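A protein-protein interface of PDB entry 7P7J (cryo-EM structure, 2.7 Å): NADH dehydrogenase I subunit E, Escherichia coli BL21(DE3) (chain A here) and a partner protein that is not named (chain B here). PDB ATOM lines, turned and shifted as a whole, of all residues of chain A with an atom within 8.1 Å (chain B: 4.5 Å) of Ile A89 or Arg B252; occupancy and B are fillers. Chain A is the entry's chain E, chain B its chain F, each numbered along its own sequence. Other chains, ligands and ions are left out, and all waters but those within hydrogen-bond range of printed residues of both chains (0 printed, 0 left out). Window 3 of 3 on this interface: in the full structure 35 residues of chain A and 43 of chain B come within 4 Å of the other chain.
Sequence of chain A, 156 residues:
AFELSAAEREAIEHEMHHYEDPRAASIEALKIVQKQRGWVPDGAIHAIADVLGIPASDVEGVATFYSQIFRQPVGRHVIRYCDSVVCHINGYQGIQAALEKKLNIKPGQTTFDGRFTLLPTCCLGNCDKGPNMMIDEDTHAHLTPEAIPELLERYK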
ATOM      1  N   ASP A  83      10.399  31.191  21.531  1.00  0.00           N
ATOM      2  CA  ASP A  83       9.492  30.421  22.369  1.00  0.00           C
ATOM      3  C   ASP A  83       8.110  30.245  21.750  1.00  0.00           C
ATOM      4  O   ASP A  83       7.189  29.797  22.437  1.00  0.00           O
ATOM      5  CB  ASP A  83       9.381  31.056  23.764  1.00  0.00           C
ATOM      6  CG  ASP A  83       8.885  32.502  23.747  1.00  0.00           C
ATOM      7  OD1 ASP A  83       8.386  33.002  22.718  1.00  0.00           O
ATOM      8  OD2 ASP A  83       8.989  33.151  24.807  1.00  0.00           O
ATOM      9  N   SER A  84       7.946  30.583  20.474  1.00  0.00           N
ATOM     10  CA  SER A  84       6.629  30.591  19.854  1.00  0.00           C
ATOM     11  C   SER A  84       6.200  29.165  19.511  1.00  0.00           C
ATOM     12  O   SER A  84       6.861  28.185  19.864  1.00  0.00           O
ATOM     13  CB  SER A  84       6.625  31.512  18.639  1.00  0.00           C
ATOM     14  OG  SER A  84       6.784  32.864  19.026  1.00  0.00           O
ATOM     15  N   VAL A  85       5.079  29.044  18.799  1.00  0.00           N
ATOM     16  CA  VAL A  85       4.338  27.786  18.766  1.00  0.00           C
ATOM     17  C   VAL A  85       5.040  26.741  17.900  1.00  0.00           C
ATOM     18  O   VAL A  85       5.127  25.567  18.281  1.00  0.00           O
ATOM     19  CB  VAL A  85       2.887  28.049  18.318  1.00  0.00           C
ATOM     20  CG1 VAL A  85       2.832  28.886  17.041  1.00  0.00           C
ATOM     21  CG2 VAL A  85       2.119  26.755  18.170  1.00  0.00           C
ATOM     22  N   VAL A  86       5.568  27.140  16.740  1.00  0.00           N
ATOM     23  CA  VAL A  86       6.180  26.169  15.836  1.00  0.00           C
ATOM     24  C   VAL A  86       7.495  25.654  16.410  1.00  0.00           C
ATOM     25  O   VAL A  86       7.814  24.466  16.293  1.00  0.00           O
ATOM     26  CB  VAL A  86       6.369  26.777  14.437  1.00  0.00           C
ATOM     27  CG1 VAL A  86       6.644  25.686  13.419  1.00  0.00           C
ATOM     28  CG2 VAL A  86       5.145  27.584  14.042  1.00  0.00           C
ATOM     29  N   CYS A  87       8.278  26.533  17.034  1.00  0.00           N
ATOM     30  CA  CYS A  87       9.492  26.085  17.702  1.00  0.00           C
ATOM     31  C   CYS A  87       9.189  25.297  18.969  1.00  0.00           C
ATOM     32  O   CYS A  87      10.014  24.478  19.387  1.00  0.00           O
ATOM     33  CB  CYS A  87      10.389  27.282  18.014  1.00  0.00           C
ATOM     34  SG  CYS A  87      10.995  28.139  16.542  1.00  0.00           S
ATOM     35  N   HIS A  88       8.031  25.530  19.590  1.00  0.00           N
ATOM     36  CA  HIS A  88       7.586  24.672  20.683  1.00  0.00           C
ATOM     37  C   HIS A  88       7.245  23.278  20.177  1.00  0.00           C
ATOM     38  O   HIS A  88       7.495  22.282  20.864  1.00  0.00           O
ATOM     39  CB  HIS A  88       6.383  25.302  21.383  1.00  0.00           C
ATOM     40  CG  HIS A  88       5.758  24.428  22.424  1.00  0.00           C
ATOM     41  ND1 HIS A  88       4.682  23.609  22.159  1.00  0.00           N
ATOM     42  CD2 HIS A  88       6.050  24.253  23.733  1.00  0.00           C
ATOM     43  CE1 HIS A  88       4.343  22.961  23.259  1.00  0.00           C
ATOM     44  NE2 HIS A  88       5.157  23.335  24.229  1.00  0.00           N
ATOM     45  N   ILE A  89       6.652  23.197  18.983  1.00  0.00           N
ATOM     46  CA  ILE A  89       6.388  21.908  18.348  1.00  0.00           C
ATOM     47  C   ILE A  89       7.695  21.189  18.043  1.00  0.00           C
ATOM     48  O   ILE A  89       7.838  19.988  18.301  1.00  0.00           O
ATOM     49  CB  ILE A  89       5.537  22.114  17.081  1.00  0.00           C
ATOM     50  CG1 ILE A  89       4.127  22.572  17.459  1.00  0.00           C
ATOM     51  CG2 ILE A  89       5.503  20.853  16.230  1.00  0.00           C
ATOM     52  CD1 ILE A  89       3.144  22.579  16.314  1.00  0.00           C
ATOM     53  N   ASN A  90       8.678  21.918  17.522  1.00  0.00           N
ATOM     54  CA  ASN A  90       9.983  21.359  17.199  1.00  0.00           C
ATOM     55  C   ASN A  90      10.912  21.281  18.404  1.00  0.00           C
ATOM     56  O   ASN A  90      12.099  20.983  18.234  1.00  0.00           O
ATOM     57  CB  ASN A  90      10.638  22.174  16.084  1.00  0.00           C
ATOM     58  CG  ASN A  90       9.848  22.131  14.794  1.00  0.00           C
ATOM     59  OD1 ASN A  90       9.490  23.168  14.237  1.00  0.00           O
ATOM     60  ND2 ASN A  90       9.566  20.928  14.314  1.00  0.00           N
ATOM     61  N   GLY A  91      10.407  21.543  19.606  1.00  0.00           N
ATOM     62  CA  GLY A  91      11.179  21.354  20.818  1.00  0.00           C
ATOM     63  C   GLY A  91      12.156  22.461  21.150  1.00  0.00           C
ATOM     64  O   GLY A  91      13.367  22.229  21.200  1.00  0.00           O
ATOM     65  N   TYR A  92      11.647  23.673  21.383  1.00  0.00           N
ATOM     66  CA  TYR A  92      12.500  24.739  21.891  1.00  0.00           C
ATOM     67  C   TYR A  92      12.815  24.562  23.369  1.00  0.00           C
ATOM     68  O   TYR A  92      13.747  25.199  23.868  1.00  0.00           O
ATOM     69  CB  TYR A  92      11.850  26.110  21.660  1.00  0.00           C
ATOM     70  CG  TYR A  92      11.068  26.648  22.845  1.00  0.00           C
ATOM     71  CD1 TYR A  92       9.770  26.222  23.091  1.00  0.00           C
ATOM     72  CD2 TYR A  92      11.620  27.592  23.707  1.00  0.00           C
ATOM     73  CE1 TYR A  92       9.050  26.704  24.165  1.00  0.00           C
ATOM     74  CE2 TYR A  92      10.910  28.069  24.790  1.00  0.00           C
ATOM     75  CZ  TYR A  92       9.623  27.628  25.008  1.00  0.00           C
ATOM     76  OH  TYR A  92       8.905  28.109  26.078  1.00  0.00           O
ATOM     77  N   GLN A  93      12.044  23.732  24.078  1.00  0.00           N
ATOM     78  CA  GLN A  93      12.232  23.584  25.517  1.00  0.00           C
ATOM     79  C   GLN A  93      13.558  22.907  25.838  1.00  0.00           C
ATOM     80  O   GLN A  93      14.216  23.261  26.823  1.00  0.00           O
ATOM     81  CB  GLN A  93      11.065  22.806  26.119  1.00  0.00           C
ATOM     82  CG  GLN A  93       9.708  23.209  25.568  1.00  0.00           C
ATOM     83  CD  GLN A  93       8.725  23.583  26.658  1.00  0.00           C
ATOM     84  OE1 GLN A  93       9.091  24.217  27.647  1.00  0.00           O
ATOM     85  NE2 GLN A  93       7.469  23.194  26.482  1.00  0.00           N
ATOM     86  N   CYS A 127      10.009  29.475  10.793  1.00  0.00           N
ATOM     87  CA  CYS A 127       9.301  28.385  11.456  1.00  0.00           C
ATOM     88  C   CYS A 127       9.467  27.061  10.726  1.00  0.00           C
ATOM     89  O   CYS A 127       9.376  25.999  11.352  1.00  0.00           O
ATOM     90  CB  CYS A 127       7.824  28.738  11.583  1.00  0.00           C
ATOM     91  SG  CYS A 127       7.547  30.478  11.928  1.00  0.00           S
ATOM     92  N   ASP A 128       9.704  27.093   9.415  1.00  0.00           N
ATOM     93  CA  ASP A 128       9.931  25.860   8.673  1.00  0.00           C
ATOM     94  C   ASP A 128      11.285  25.235   8.978  1.00  0.00           C
ATOM     95  O   ASP A 128      11.509  24.074   8.618  1.00  0.00           O
ATOM     96  CB  ASP A 128       9.806  26.118   7.171  1.00  0.00           C
ATOM     97  CG  ASP A 128      10.586  27.332   6.722  1.00  0.00           C
ATOM     98  OD1 ASP A 128      11.071  28.084   7.592  1.00  0.00           O
ATOM     99  OD2 ASP A 128      10.719  27.537   5.498  1.00  0.00           O
ATOM    100  N   GLY A 130      12.580  25.422  12.262  1.00  0.00           N
ATOM    101  CA  GLY A 130      12.610  25.515  13.702  1.00  0.00           C
ATOM    102  C   GLY A 130      13.256  24.316  14.365  1.00  0.00           C
ATOM    103  O   GLY A 130      13.331  23.228  13.785  1.00  0.00           O
ATOM    104  N   PRO A 131      13.745  24.486  15.607  1.00  0.00           N
ATOM    105  CA  PRO A 131      13.754  25.719  16.406  1.00  0.00           C
ATOM    106  C   PRO A 131      14.834  26.712  15.984  1.00  0.00           C
ATOM    107  O   PRO A 131      15.827  26.316  15.376  1.00  0.00           O
ATOM    108  CB  PRO A 131      14.015  25.210  17.823  1.00  0.00           C
ATOM    109  CG  PRO A 131      14.800  23.975  17.626  1.00  0.00           C
ATOM    110  CD  PRO A 131      14.279  23.342  16.367  1.00  0.00           C
ATOM    111  N   SER B 250       3.991  23.422   8.028  1.00  0.00           N
ATOM    112  CA  SER B 250       5.173  23.447   8.871  1.00  0.00           C
ATOM    113  C   SER B 250       4.889  22.728  10.181  1.00  0.00           C
ATOM    114  O   SER B 250       3.752  22.694  10.658  1.00  0.00           O
ATOM    115  CB  SER B 250       5.633  24.880   9.157  1.00  0.00           C
ATOM    116  OG  SER B 250       4.656  25.588   9.899  1.00  0.00           O
ATOM    117  N   GLY B 251       5.940  22.156  10.755  1.00  0.00           N
ATOM    118  CA  GLY B 251       5.863  21.544  12.065  1.00  0.00           C
ATOM    119  C   GLY B 251       5.840  20.031  12.047  1.00  0.00           C
ATOM    120  O   GLY B 251       4.779  19.423  11.870  1.00  0.00           O
ATOM    121  N   ARG B 252       7.016  19.430  12.259  1.00  0.00           N
ATOM    122  CA  ARG B 252       7.197  17.980  12.398  1.00  0.00           C
ATOM    123  C   ARG B 252       6.630  17.203  11.210  1.00  0.00           C
ATOM    124  O   ARG B 252       6.014  16.149  11.371  1.00  0.00           O
ATOM    125  CB  ARG B 252       6.603  17.476  13.715  1.00  0.00           C
ATOM    126  CG  ARG B 252       7.549  17.642  14.894  1.00  0.00           C
ATOM    127  CD  ARG B 252       6.863  17.356  16.216  1.00  0.00           C
ATOM    128  NE  ARG B 252       7.535  16.295  16.955  1.00  0.00           N
ATOM    129  CZ  ARG B 252       6.988  15.616  17.954  1.00  0.00           C
ATOM    130  NH1 ARG B 252       5.756  15.863  18.363  1.00  0.00           N
ATOM    131  NH2 ARG B 252       7.698  14.669  18.558  1.00  0.00           N
ATOM    132  N   VAL B 253       6.843  17.726  10.007  1.00  0.00           N
ATOM    133  CA  VAL B 253       6.450  17.048   8.784  1.00  0.00           C
ATOM    134  C   VAL B 253       7.711  16.644   8.026  1.00  0.00           C
ATOM    135  O   VAL B 253       8.829  16.991   8.403  1.00  0.00           O
ATOM    136  CB  VAL B 253       5.524  17.915   7.910  1.00  0.00           C
ATOM    137  CG1 VAL B 253       4.158  18.037   8.553  1.00  0.00           C
ATOM    138  CG2 VAL B 253       6.132  19.283   7.696  1.00  0.00           C
ATOM    139  N   MET B 278       3.185  13.610   7.588  1.00  0.00           N
ATOM    140  CA  MET B 278       3.835  13.748   8.879  1.00  0.00           C
ATOM    141  C   MET B 278       5.122  12.927   8.914  1.00  0.00           C
ATOM    142  O   MET B 278       5.399  12.110   8.032  1.00  0.00           O
ATOM    143  CB  MET B 278       2.892  13.319  10.002  1.00  0.00           C
ATOM    144  CG  MET B 278       1.573  14.070  10.015  1.00  0.00           C
ATOM    145  SD  MET B 278       1.639  15.655  10.874  1.00  0.00           S
ATOM    146  CE  MET B 278       2.891  15.349  12.113  1.00  0.00           C
ATOM    147  N   ARG B 279       5.916  13.152   9.956  1.00  0.00           N
ATOM    148  CA  ARG B 279       7.178  12.446  10.104  1.00  0.00           C
ATOM    149  C   ARG B 279       6.927  11.007  10.555  1.00  0.00           C
ATOM    150  O   ARG B 279       5.786  10.570  10.732  1.00  0.00           O
ATOM    151  CB  ARG B 279       8.093  13.187  11.077  1.00  0.00           C
ATOM    152  CG  ARG B 279       9.534  13.283  10.602  1.00  0.00           C
ATOM    153  CD  ARG B 279      10.458  13.841  11.672  1.00  0.00           C
ATOM    154  NE  ARG B 279      10.609  15.287  11.580  1.00  0.00           N
ATOM    155  CZ  ARG B 279      10.459  16.124  12.599  1.00  0.00           C
ATOM    156  NH1 ARG B 279      10.162  15.689  13.812  1.00  0.00           N
ATOM    157  NH2 ARG B 279      10.617  17.428  12.395  1.00  0.00           N
ATOM    158  N   LEU B 282       4.361   9.404  13.686  1.00  0.00           N
ATOM    159  CA  LEU B 282       3.597  10.523  14.218  1.00  0.00           C
ATOM    160  C   LEU B 282       2.191  10.488  13.645  1.00  0.00           C
ATOM    161  O   LEU B 282       2.016  10.440  12.424  1.00  0.00           O
ATOM    162  CB  LEU B 282       4.269  11.861  13.896  1.00  0.00           C
ATOM    163  CG  LEU B 282       5.613  12.121  14.578  1.00  0.00           C
ATOM    164  CD1 LEU B 282       6.117  13.516  14.254  1.00  0.00           C
ATOM    165  CD2 LEU B 282       5.503  11.929  16.081  1.00  0.00           C
ATOM    166  N   MET B 324       0.126  24.952   9.959  1.00  0.00           N
ATOM    167  CA  MET B 324       1.010  24.303  10.915  1.00  0.00           C
ATOM    168  C   MET B 324       0.324  23.058  11.452  1.00  0.00           C
ATOM    169  O   MET B 324      -0.839  23.115  11.859  1.00  0.00           O
ATOM    170  CB  MET B 324       1.389  25.265  12.041  1.00  0.00           C
ATOM    171  CG  MET B 324       1.832  24.612  13.327  1.00  0.00           C
ATOM    172  SD  MET B 324       1.583  25.753  14.693  1.00  0.00           S
ATOM    173  CE  MET B 324       0.251  24.945  15.563  1.00  0.00           C
ATOM    174  N   ALA B 325       1.044  21.940  11.443  1.00  0.00           N
ATOM    175  CA  ALA B 325       0.487  20.640  11.786  1.00  0.00           C
ATOM    176  C   ALA B 325       0.906  20.222  13.189  1.00  0.00           C
ATOM    177  O   ALA B 325       2.070  20.369  13.571  1.00  0.00           O
ATOM    178  CB  ALA B 325       0.926  19.579  10.777  1.00  0.00           C
ATOM    179  N   VAL B 326      -0.052  19.698  13.949  1.00  0.00           N
ATOM    180  CA  VAL B 326       0.151  19.225  15.311  1.00  0.00           C
ATOM    181  C   VAL B 326      -0.126  17.731  15.333  1.00  0.00           C
ATOM    182  O   VAL B 326      -1.204  17.294  14.912  1.00  0.00           O
ATOM    183  CB  VAL B 326      -0.771  19.953  16.305  1.00  0.00           C
ATOM    184  CG1 VAL B 326      -0.603  19.390  17.701  1.00  0.00           C
ATOM    185  CG2 VAL B 326      -0.490  21.426  16.287  1.00  0.00           C
ATOM    186  N   ASP B 327       0.832  16.960  15.837  1.00  0.00           N
ATOM    187  CA  ASP B 327       0.702  15.515  15.912  1.00  0.00           C
ATOM    188  C   ASP B 327       0.113  15.104  17.260  1.00  0.00           C
ATOM    189  O   ASP B 327      -0.273  15.937  18.081  1.00  0.00           O
ATOM    190  CB  ASP B 327       2.051  14.847  15.663  1.00  0.00           C
ATOM    191  CG  ASP B 327       3.165  15.478  16.460  1.00  0.00           C
ATOM    192  OD1 ASP B 327       3.279  16.719  16.431  1.00  0.00           O
ATOM    193  OD2 ASP B 327       3.925  14.738  17.118  1.00  0.00           O
ATOM    194  N   GLU B 329       1.616  13.609  19.746  1.00  0.00           N
ATOM    195  CA  GLU B 329       2.529  13.713  20.879  1.00  0.00           C
ATOM    196  C   GLU B 329       2.337  15.013  21.652  1.00  0.00           C
ATOM    197  O   GLU B 329       2.620  15.067  22.853  1.00  0.00           O
ATOM    198  CB  GLU B 329       3.973  13.587  20.388  1.00  0.00           C
ATOM    199  CG  GLU B 329       5.005  13.372  21.483  1.00  0.00           C
ATOM    200  CD  GLU B 329       4.834  12.046  22.196  1.00  0.00           C
ATOM    201  OE1 GLU B 329       4.472  11.053  21.529  1.00  0.00           O
ATOM    202  OE2 GLU B 329       5.061  11.995  23.423  1.00  0.00           O
ATOM    203  N   ILE B 330       1.847  16.056  20.994  1.00  0.00           N
ATOM    204  CA  ILE B 330       1.746  17.372  21.611  1.00  0.00           C
ATOM    205  C   ILE B 330       0.469  17.458  22.434  1.00  0.00           C
ATOM    206  O   ILE B 330      -0.628  17.180  21.934  1.00  0.00           O
ATOM    207  CB  ILE B 330       1.788  18.474  20.543  1.00  0.00           C
ATOM    208  CG1 ILE B 330       3.034  18.315  19.680  1.00  0.00           C
ATOM    209  CG2 ILE B 330       1.762  19.846  21.187  1.00  0.00           C
ATOM    210  CD1 ILE B 330       3.059  19.236  18.510  1.00  0.00           C
ATOM    211  N   LEU B 335       0.169  23.559  24.214  1.00  0.00           N
ATOM    212  CA  LEU B 335       0.293  24.333  22.983  1.00  0.00           C
ATOM    213  C   LEU B 335      -0.541  25.606  23.040  1.00  0.00           C
ATOM    214  O   LEU B 335      -0.069  26.690  22.676  1.00  0.00           O
ATOM    215  CB  LEU B 335      -0.121  23.477  21.791  1.00  0.00           C
ATOM    216  CG  LEU B 335       0.297  24.007  20.425  1.00  0.00           C
ATOM    217  CD1 LEU B 335       1.731  23.622  20.138  1.00  0.00           C
ATOM    218  CD2 LEU B 335      -0.627  23.465  19.366  1.00  0.00           C
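The side-chain amide oxygen (OD1) of Asn A90 sits close to the backbone carbonyl oxygen (O) of Val A86, at 3.0 Å.
The backbone carbonyl oxygen of Arg B252 lies within hydrogen-bond range of the backbone NH of Arg B279, at 3.3 Å.
The backbone carbonyl oxygen of Ser B250 lies within hydrogen-bond range of the backbone NH of Ala B325 (2.9 Å).
NE2 of Gln A93 lies within hydrogen-bond range of NE2 of His A88 (3.2 Å).
The guanidinium group of Arg B252 is in salt-bridge range of the side-chain carboxylate of Asp B327 (2.5 Å).
Val A85 touches Met B324.
CD1 of Leu B335 touches CG2 of Val A85 (3.7 Å).
His A88 touches Leu B335 (ND1 to CD1, 3.6 Å).
Ile A89 touches Arg B252.
Met B324 touches Ile A89.
Ala B325 touches Ile A89 (O to CD1, 3.7 Å).
CD1 of Ile A89 touches CG2 of Val B326, 3.8 Å away.
Ile B330 touches Ile A89.
CG1 of Ile A89 touches CD1 of Leu B335, 3.7 Å away.
Arg B252 touches Asn A90.
Of the 14 printed residues of chain B, 6 touch a printed residue of chain A.
Printed residues of chain B that touch a printed residue of chain A: Arg B252, Met B324, Ala B325, Val B326, Ile B330 and Leu B335.
Of the 15 printed residues of chain A, 4 touch a printed residue of chain B.
Hydrophobic or aromatic side chains of chain A that line the printed part of chain B: Val A85, His A88 and Ile A89.
Among the printed residues, 10 pairs touch across the chains.
Ile A89 touches just these residues of chain B: Arg B252 (3.5 Å), Met B324 (3.8 Å), Ala B325 (3.7 Å), Val B326 (3.8 Å), Ile B330 (3.7 Å) and Leu B335 (3.7 Å).
Of chain A, only Ile A89 and Asn A90 come within 4 Å of Arg B252.
Gly B251 touches none of the printed residues of chain A.
Printed residues of chain A within 4 Å of Ile B330: Ile A89 (3.7 Å).
Of the printed residues of chain B, His A88 touches Leu B335 (3.6 Å).
Of the printed residues of chain A, Leu B335 touches Val A85, His A88 and Ile A89.
Of the printed residues of chain A, Val B326 touches Ile A89 (3.8 Å).
Of the printed residues of chain A, Ala B325 touches Ile A89 (3.7 Å).
Ser A84 touches none of the printed residues of chain B.
Gly A130 touches none of the printed residues of chain B.
The nearest residue of chain B that does not touch Ile A89 is Gly B251 (4.2 Å).
The nearest residue of chain A that does not touch Arg B252 is Val A86 (6.4 Å).
The nearest printed residue of chain A that does not touch Met B324 is Val A86 (4.1 Å).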
